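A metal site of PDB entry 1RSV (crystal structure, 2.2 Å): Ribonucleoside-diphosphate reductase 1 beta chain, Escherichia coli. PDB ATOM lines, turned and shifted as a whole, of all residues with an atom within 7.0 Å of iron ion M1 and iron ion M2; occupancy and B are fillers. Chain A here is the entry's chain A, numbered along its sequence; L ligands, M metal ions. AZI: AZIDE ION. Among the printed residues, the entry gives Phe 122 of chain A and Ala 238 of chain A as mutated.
Merely in contact with iron ion M1: Phe 208 (3.7 Å). Within 4 Å of iron ion M1: Asp 84, Glu 115, His 118 and Phe 208. The nearest printed residue that does not touch iron ion M1 is Ile 234 (4.4 Å).
Iron ion M2 is bound by the side-chain carboxylate (OE2) of Glu 115 (2.0 Å), a ring nitrogen (ND1) of His 241 (2.0 Å), a nitrogen (N1) of the ligand (2.0 Å), the side-chain carboxylate (OE2) of Glu 204 (2.3 Å) and the side-chain carboxylate (OE1) of Glu 204 (2.3 Å).
OG of Ser 114 is in hydrogen-bond range of O of Trp 111, at 2.6 Å. NE2 of His 118 lies within hydrogen-bond range of OD2 of Asp 237, at 2.5 Å. OE2 of Glu 204 sits close to NE1 of Trp 111, 3.4 Å away. OE2 of Glu 115 sits close to NE1 of Trp 111, 3.2 Å away. The indole nitrogen (NE1) of Trp 111 lies close to a ring nitrogen (ND1) of His 241. The backbone carbonyl oxygen (O) of Glu 115 lies within hydrogen-bond range of the side-chain hydroxyl (OG) of Ser 119, at 3.3 Å. The side-chain carboxylate (OE2) of Glu 204 lies close to the side-chain amide oxygen (OE1) of Gln 87 (3.2 Å). The side-chain hydroxyl (OG) of Ser 114 lies within hydrogen-bond range of a ring nitrogen (NE2) of His 241 (2.9 Å).
Residues that only touch iron ion M2: Trp 111 (3.9 Å).
Iron ion M1 is bound by the side-chain carboxylate (OD1) of Asp 84 (1.9 Å), the side-chain carboxylate (OE1) of Glu 115 (2.0 Å), a ring nitrogen (ND1) of His 118 (2.1 Å) and a nitrogen (N1) of the ligand (2.3 Å).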
ATOM      1  N   GLN A  80      12.150 -21.153  18.749  1.00  0.00           N
ATOM      2  CA  GLN A  80      11.255 -21.537  17.677  1.00  0.00           C
ATOM      3  C   GLN A  80      11.405 -23.061  17.431  1.00  0.00           C
ATOM      4  O   GLN A  80      10.432 -23.816  17.345  1.00  0.00           O
ATOM      5  CB  GLN A  80      11.686 -20.770  16.416  1.00  0.00           C
ATOM      6  CG  GLN A  80      11.618 -19.252  16.620  1.00  0.00           C
ATOM      7  CD  GLN A  80      12.074 -18.439  15.387  1.00  0.00           C
ATOM      8  OE1 GLN A  80      13.178 -18.598  14.830  1.00  0.00           O
ATOM      9  NE2 GLN A  80      11.207 -17.523  14.970  1.00  0.00           N
ATOM     10  N   LEU A  83       9.664 -25.125  19.966  1.00  0.00           N
ATOM     11  CA  LEU A  83       8.223 -25.170  19.798  1.00  0.00           C
ATOM     12  C   LEU A  83       7.743 -26.022  18.626  1.00  0.00           C
ATOM     13  O   LEU A  83       6.684 -26.663  18.700  1.00  0.00           O
ATOM     14  CB  LEU A  83       7.589 -23.767  19.717  1.00  0.00           C
ATOM     15  CG  LEU A  83       7.665 -22.815  20.937  1.00  0.00           C
ATOM     16  CD1 LEU A  83       6.906 -21.522  20.637  1.00  0.00           C
ATOM     17  CD2 LEU A  83       7.151 -23.463  22.209  1.00  0.00           C
ATOM     18  N   ASP A  84       8.514 -26.005  17.530  1.00  0.00           N
ATOM     19  CA  ASP A  84       8.128 -26.798  16.352  1.00  0.00           C
ATOM     20  C   ASP A  84       8.431 -28.241  16.618  1.00  0.00           C
ATOM     21  O   ASP A  84       7.725 -29.065  16.120  1.00  0.00           O
ATOM     22  CB  ASP A  84       8.683 -26.239  15.061  1.00  0.00           C
ATOM     23  CG  ASP A  84       7.839 -25.065  14.569  1.00  0.00           C
ATOM     24  OD1 ASP A  84       6.639 -25.124  14.548  1.00  0.00           O
ATOM     25  OD2 ASP A  84       8.433 -23.982  14.170  1.00  0.00           O
ATOM     26  N   GLN A  87       5.336 -29.204  18.411  1.00  0.00           N
ATOM     27  CA  GLN A  87       4.162 -29.095  17.546  1.00  0.00           C
ATOM     28  C   GLN A  87       4.138 -30.076  16.378  1.00  0.00           C
ATOM     29  O   GLN A  87       3.141 -30.237  15.725  1.00  0.00           O
ATOM     30  CB  GLN A  87       4.087 -27.669  16.953  1.00  0.00           C
ATOM     31  CG  GLN A  87       3.715 -26.639  18.035  1.00  0.00           C
ATOM     32  CD  GLN A  87       2.369 -26.933  18.622  1.00  0.00           C
ATOM     33  OE1 GLN A  87       1.346 -26.511  18.102  1.00  0.00           O
ATOM     34  NE2 GLN A  87       2.361 -27.679  19.672  1.00  0.00           N
ATOM     35  N   TRP A 111      -1.721 -30.189   9.748  1.00  0.00           N
ATOM     36  CA  TRP A 111      -1.182 -29.178  10.593  1.00  0.00           C
ATOM     37  C   TRP A 111       0.080 -29.679  11.183  1.00  0.00           C
ATOM     38  O   TRP A 111       1.121 -29.063  11.088  1.00  0.00           O
ATOM     39  CB  TRP A 111      -2.252 -28.851  11.658  1.00  0.00           C
ATOM     40  CG  TRP A 111      -1.831 -28.005  12.843  1.00  0.00           C
ATOM     41  CD1 TRP A 111      -0.702 -27.218  12.974  1.00  0.00           C
ATOM     42  CD2 TRP A 111      -2.549 -27.899  14.094  1.00  0.00           C
ATOM     43  NE1 TRP A 111      -0.696 -26.636  14.232  1.00  0.00           N
ATOM     44  CE2 TRP A 111      -1.835 -27.006  14.909  1.00  0.00           C
ATOM     45  CE3 TRP A 111      -3.736 -28.440  14.581  1.00  0.00           C
ATOM     46  CZ2 TRP A 111      -2.255 -26.676  16.198  1.00  0.00           C
ATOM     47  CZ3 TRP A 111      -4.180 -28.071  15.855  1.00  0.00           C
ATOM     48  CH2 TRP A 111      -3.412 -27.214  16.658  1.00  0.00           C
ATOM     49  N   SER A 114       2.686 -29.933   8.689  1.00  0.00           N
ATOM     50  CA  SER A 114       3.212 -28.608   8.348  1.00  0.00           C
ATOM     51  C   SER A 114       4.283 -28.164   9.324  1.00  0.00           C
ATOM     52  O   SER A 114       5.222 -27.490   9.000  1.00  0.00           O
ATOM     53  CB  SER A 114       2.074 -27.566   8.256  1.00  0.00           C
ATOM     54  OG  SER A 114       1.742 -27.127   9.532  1.00  0.00           O
ATOM     55  N   GLU A 115       4.143 -28.558  10.586  1.00  0.00           N
ATOM     56  CA  GLU A 115       5.125 -28.222  11.618  1.00  0.00           C
ATOM     57  C   GLU A 115       6.456 -28.962  11.441  1.00  0.00           C
ATOM     58  O   GLU A 115       7.558 -28.404  11.716  1.00  0.00           O
ATOM     59  CB  GLU A 115       4.540 -28.527  13.019  1.00  0.00           C
ATOM     60  CG  GLU A 115       3.178 -27.801  13.380  1.00  0.00           C
ATOM     61  CD  GLU A 115       3.280 -26.279  13.588  1.00  0.00           C
ATOM     62  OE1 GLU A 115       4.190 -25.597  13.093  1.00  0.00           O
ATOM     63  OE2 GLU A 115       2.340 -25.701  14.298  1.00  0.00           O
ATOM     64  N   THR A 116       6.404 -30.262  10.998  1.00  0.00           N
ATOM     65  CA  THR A 116       7.657 -31.018  10.798  1.00  0.00           C
ATOM     66  C   THR A 116       8.460 -30.286   9.749  1.00  0.00           C
ATOM     67  O   THR A 116       9.677 -30.281   9.772  1.00  0.00           O
ATOM     68  CB  THR A 116       7.443 -32.499  10.389  1.00  0.00           C
ATOM     69  OG1 THR A 116       6.685 -32.557   9.188  1.00  0.00           O
ATOM     70  CG2 THR A 116       6.706 -33.216  11.531  1.00  0.00           C
ATOM     71  N   ILE A 117       7.767 -29.678   8.823  1.00  0.00           N
ATOM     72  CA  ILE A 117       8.413 -28.891   7.785  1.00  0.00           C
ATOM     73  C   ILE A 117       9.085 -27.684   8.446  1.00  0.00           C
ATOM     74  O   ILE A 117      10.221 -27.346   8.116  1.00  0.00           O
ATOM     75  CB  ILE A 117       7.385 -28.429   6.734  1.00  0.00           C
ATOM     76  CG1 ILE A 117       6.776 -29.651   6.010  1.00  0.00           C
ATOM     77  CG2 ILE A 117       8.096 -27.585   5.675  1.00  0.00           C
ATOM     78  CD1 ILE A 117       7.789 -30.310   5.090  1.00  0.00           C
ATOM     79  N   HIS A 118       8.384 -27.027   9.393  1.00  0.00           N
ATOM     80  CA  HIS A 118       8.960 -25.872  10.124  1.00  0.00           C
ATOM     81  C   HIS A 118      10.258 -26.354  10.798  1.00  0.00           C
ATOM     82  O   HIS A 118      11.332 -25.762  10.733  1.00  0.00           O
ATOM     83  CB  HIS A 118       7.919 -25.251  11.150  1.00  0.00           C
ATOM     84  CG  HIS A 118       6.681 -24.684  10.525  1.00  0.00           C
ATOM     85  ND1 HIS A 118       5.545 -24.348  11.256  1.00  0.00           N
ATOM     86  CD2 HIS A 118       6.400 -24.400   9.236  1.00  0.00           C
ATOM     87  CE1 HIS A 118       4.616 -23.906  10.426  1.00  0.00           C
ATOM     88  NE2 HIS A 118       5.101 -23.915   9.191  1.00  0.00           N
ATOM     89  N   SER A 119      10.181 -27.505  11.421  1.00  0.00           N
ATOM     90  CA  SER A 119      11.381 -27.992  12.015  1.00  0.00           C
ATOM     91  C   SER A 119      12.503 -28.248  11.000  1.00  0.00           C
ATOM     92  O   SER A 119      13.663 -27.941  11.237  1.00  0.00           O
ATOM     93  CB  SER A 119      11.122 -29.252  12.813  1.00  0.00           C
ATOM     94  OG  SER A 119      10.122 -28.998  13.774  1.00  0.00           O
ATOM     95  N   PHE A 122      14.352 -25.150  10.265  1.00  0.00           N
ATOM     96  CA  PHE A 122      15.319 -24.681  11.274  1.00  0.00           C
ATOM     97  C   PHE A 122      16.667 -25.403  11.196  1.00  0.00           C
ATOM     98  O   PHE A 122      17.729 -24.831  11.349  1.00  0.00           O
ATOM     99  CB  PHE A 122      14.696 -24.812  12.665  1.00  0.00           C
ATOM    100  CG  PHE A 122      13.526 -23.884  12.814  1.00  0.00           C
ATOM    101  CD1 PHE A 122      12.317 -24.320  13.349  1.00  0.00           C
ATOM    102  CD2 PHE A 122      13.610 -22.558  12.416  1.00  0.00           C
ATOM    103  CE1 PHE A 122      11.235 -23.461  13.466  1.00  0.00           C
ATOM    104  CE2 PHE A 122      12.537 -21.684  12.533  1.00  0.00           C
ATOM    105  CZ  PHE A 122      11.339 -22.133  13.068  1.00  0.00           C
ATOM    106  N   LEU A 203      -0.012 -20.586  22.121  1.00  0.00           N
ATOM    107  CA  LEU A 203       1.266 -20.967  21.598  1.00  0.00           C
ATOM    108  C   LEU A 203       1.380 -20.494  20.165  1.00  0.00           C
ATOM    109  O   LEU A 203       2.332 -19.762  19.827  1.00  0.00           O
ATOM    110  CB  LEU A 203       1.432 -22.506  21.658  1.00  0.00           C
ATOM    111  CG  LEU A 203       2.810 -23.088  21.295  1.00  0.00           C
ATOM    112  CD1 LEU A 203       2.934 -24.576  21.699  1.00  0.00           C
ATOM    113  CD2 LEU A 203       3.061 -22.942  19.798  1.00  0.00           C
ATOM    114  N   GLU A 204       0.421 -20.888  19.311  1.00  0.00           N
ATOM    115  CA  GLU A 204       0.412 -20.478  17.870  1.00  0.00           C
ATOM    116  C   GLU A 204       0.238 -18.942  17.655  1.00  0.00           C
ATOM    117  O   GLU A 204       0.836 -18.286  16.759  1.00  0.00           O
ATOM    118  CB  GLU A 204      -0.816 -21.098  17.169  1.00  0.00           C
ATOM    119  CG  GLU A 204      -0.710 -22.598  16.979  1.00  0.00           C
ATOM    120  CD  GLU A 204       0.331 -22.935  15.921  1.00  0.00           C
ATOM    121  OE1 GLU A 204       0.662 -22.137  15.032  1.00  0.00           O
ATOM    122  OE2 GLU A 204       0.803 -24.142  15.995  1.00  0.00           O
ATOM    123  N   PHE A 208       4.657 -17.714  19.107  1.00  0.00           N
ATOM    124  CA  PHE A 208       5.357 -17.658  17.833  1.00  0.00           C
ATOM    125  C   PHE A 208       5.515 -16.241  17.265  1.00  0.00           C
ATOM    126  O   PHE A 208       6.545 -15.911  16.671  1.00  0.00           O
ATOM    127  CB  PHE A 208       4.639 -18.569  16.834  1.00  0.00           C
ATOM    128  CG  PHE A 208       5.265 -19.961  16.730  1.00  0.00           C
ATOM    129  CD1 PHE A 208       6.636 -20.143  16.518  1.00  0.00           C
ATOM    130  CD2 PHE A 208       4.460 -21.092  16.850  1.00  0.00           C
ATOM    131  CE1 PHE A 208       7.161 -21.439  16.432  1.00  0.00           C
ATOM    132  CE2 PHE A 208       4.983 -22.367  16.757  1.00  0.00           C
ATOM    133  CZ  PHE A 208       6.335 -22.558  16.537  1.00  0.00           C
ATOM    134  N   PHE A 212       8.497 -14.217  15.893  1.00  0.00           N
ATOM    135  CA  PHE A 212       8.641 -13.661  14.537  1.00  0.00           C
ATOM    136  C   PHE A 212       9.211 -12.240  14.536  1.00  0.00           C
ATOM    137  O   PHE A 212       9.989 -11.849  13.647  1.00  0.00           O
ATOM    138  CB  PHE A 212       7.285 -13.642  13.755  1.00  0.00           C
ATOM    139  CG  PHE A 212       6.704 -15.017  13.536  1.00  0.00           C
ATOM    140  CD1 PHE A 212       7.509 -16.145  13.630  1.00  0.00           C
ATOM    141  CD2 PHE A 212       5.347 -15.169  13.258  1.00  0.00           C
ATOM    142  CE1 PHE A 212       6.955 -17.410  13.460  1.00  0.00           C
ATOM    143  CE2 PHE A 212       4.782 -16.435  13.116  1.00  0.00           C
ATOM    144  CZ  PHE A 212       5.597 -17.554  13.217  1.00  0.00           C
ATOM    145  N   ILE A 234       6.692 -19.568   7.316  1.00  0.00           N
ATOM    146  CA  ILE A 234       6.214 -20.084   8.573  1.00  0.00           C
ATOM    147  C   ILE A 234       5.096 -19.237   9.100  1.00  0.00           C
ATOM    148  O   ILE A 234       4.035 -19.795   9.420  1.00  0.00           O
ATOM    149  CB  ILE A 234       7.313 -20.176   9.613  1.00  0.00           C
ATOM    150  CG1 ILE A 234       8.289 -21.215   9.165  1.00  0.00           C
ATOM    151  CG2 ILE A 234       6.755 -20.542  11.008  1.00  0.00           C
ATOM    152  CD1 ILE A 234       8.948 -21.908  10.318  1.00  0.00           C
ATOM    153  N   ASP A 237       1.980 -20.058   7.730  1.00  0.00           N
ATOM    154  CA  ASP A 237       1.361 -21.285   8.201  1.00  0.00           C
ATOM    155  C   ASP A 237       0.726 -21.027   9.537  1.00  0.00           C
ATOM    156  O   ASP A 237      -0.425 -21.397   9.782  1.00  0.00           O
ATOM    157  CB  ASP A 237       2.428 -22.419   8.335  1.00  0.00           C
ATOM    158  CG  ASP A 237       2.877 -22.911   6.957  1.00  0.00           C
ATOM    159  OD1 ASP A 237       2.214 -22.657   5.923  1.00  0.00           O
ATOM    160  OD2 ASP A 237       4.006 -23.578   6.966  1.00  0.00           O
ATOM    161  N   ALA A 238       1.475 -20.371  10.398  1.00  0.00           N
ATOM    162  CA  ALA A 238       0.984 -20.041  11.721  1.00  0.00           C
ATOM    163  C   ALA A 238      -0.360 -19.334  11.658  1.00  0.00           C
ATOM    164  O   ALA A 238      -1.277 -19.628  12.430  1.00  0.00           O
ATOM    165  CB  ALA A 238       1.992 -19.153  12.393  1.00  0.00           C
ATOM    166  N   ALA A 239      -0.532 -18.429  10.695  1.00  0.00           N
ATOM    167  CA  ALA A 239      -1.849 -17.777  10.577  1.00  0.00           C
ATOM    168  C   ALA A 239      -2.959 -18.818  10.350  1.00  0.00           C
ATOM    169  O   ALA A 239      -4.079 -18.683  10.858  1.00  0.00           O
ATOM    170  CB  ALA A 239      -1.887 -16.695   9.507  1.00  0.00           C
ATOM    171  N   HIS A 241      -2.844 -21.977  11.371  1.00  0.00           N
ATOM    172  CA  HIS A 241      -2.959 -22.774  12.589  1.00  0.00           C
ATOM    173  C   HIS A 241      -3.846 -22.100  13.638  1.00  0.00           C
ATOM    174  O   HIS A 241      -4.733 -22.729  14.210  1.00  0.00           O
ATOM    175  CB  HIS A 241      -1.559 -23.062  13.150  1.00  0.00           C
ATOM    176  CG  HIS A 241      -0.649 -23.789  12.186  1.00  0.00           C
ATOM    177  ND1 HIS A 241       0.691 -24.037  12.483  1.00  0.00           N
ATOM    178  CD2 HIS A 241      -0.901 -24.326  10.951  1.00  0.00           C
ATOM    179  CE1 HIS A 241       1.225 -24.714  11.449  1.00  0.00           C
ATOM    180  NE2 HIS A 241       0.283 -24.880  10.521  1.00  0.00           N
ATOM    181  N   LEU A 242      -3.599 -20.803  13.923  1.00  0.00           N
ATOM    182  CA  LEU A 242      -4.383 -20.140  14.939  1.00  0.00           C
ATOM    183  C   LEU A 242      -5.802 -19.967  14.450  1.00  0.00           C
ATOM    184  O   LEU A 242      -6.776 -19.925  15.245  1.00  0.00           O
ATOM    185  CB  LEU A 242      -3.752 -18.792  15.308  1.00  0.00           C
ATOM    186  CG  LEU A 242      -3.885 -17.684  14.300  1.00  0.00           C
ATOM    187  CD1 LEU A 242      -5.128 -16.854  14.640  1.00  0.00           C
ATOM    188  CD2 LEU A 242      -2.609 -16.854  14.419  1.00  0.00           C
HETATM  189  N1  AZI L   1       3.525 -23.332  12.888  1.00  0.00           N
HETATM  190  N2  AZI L   1       3.927 -22.306  13.398  1.00  0.00           N
HETATM  191  N3  AZI L   1       4.307 -21.346  13.916  1.00  0.00           N
HETATM  192 FE    FE M   1       5.587 -24.140  13.333  1.00  0.00          FE
HETATM  193 FE    FE M   2       1.922 -23.765  14.073  1.00  0.00          FE
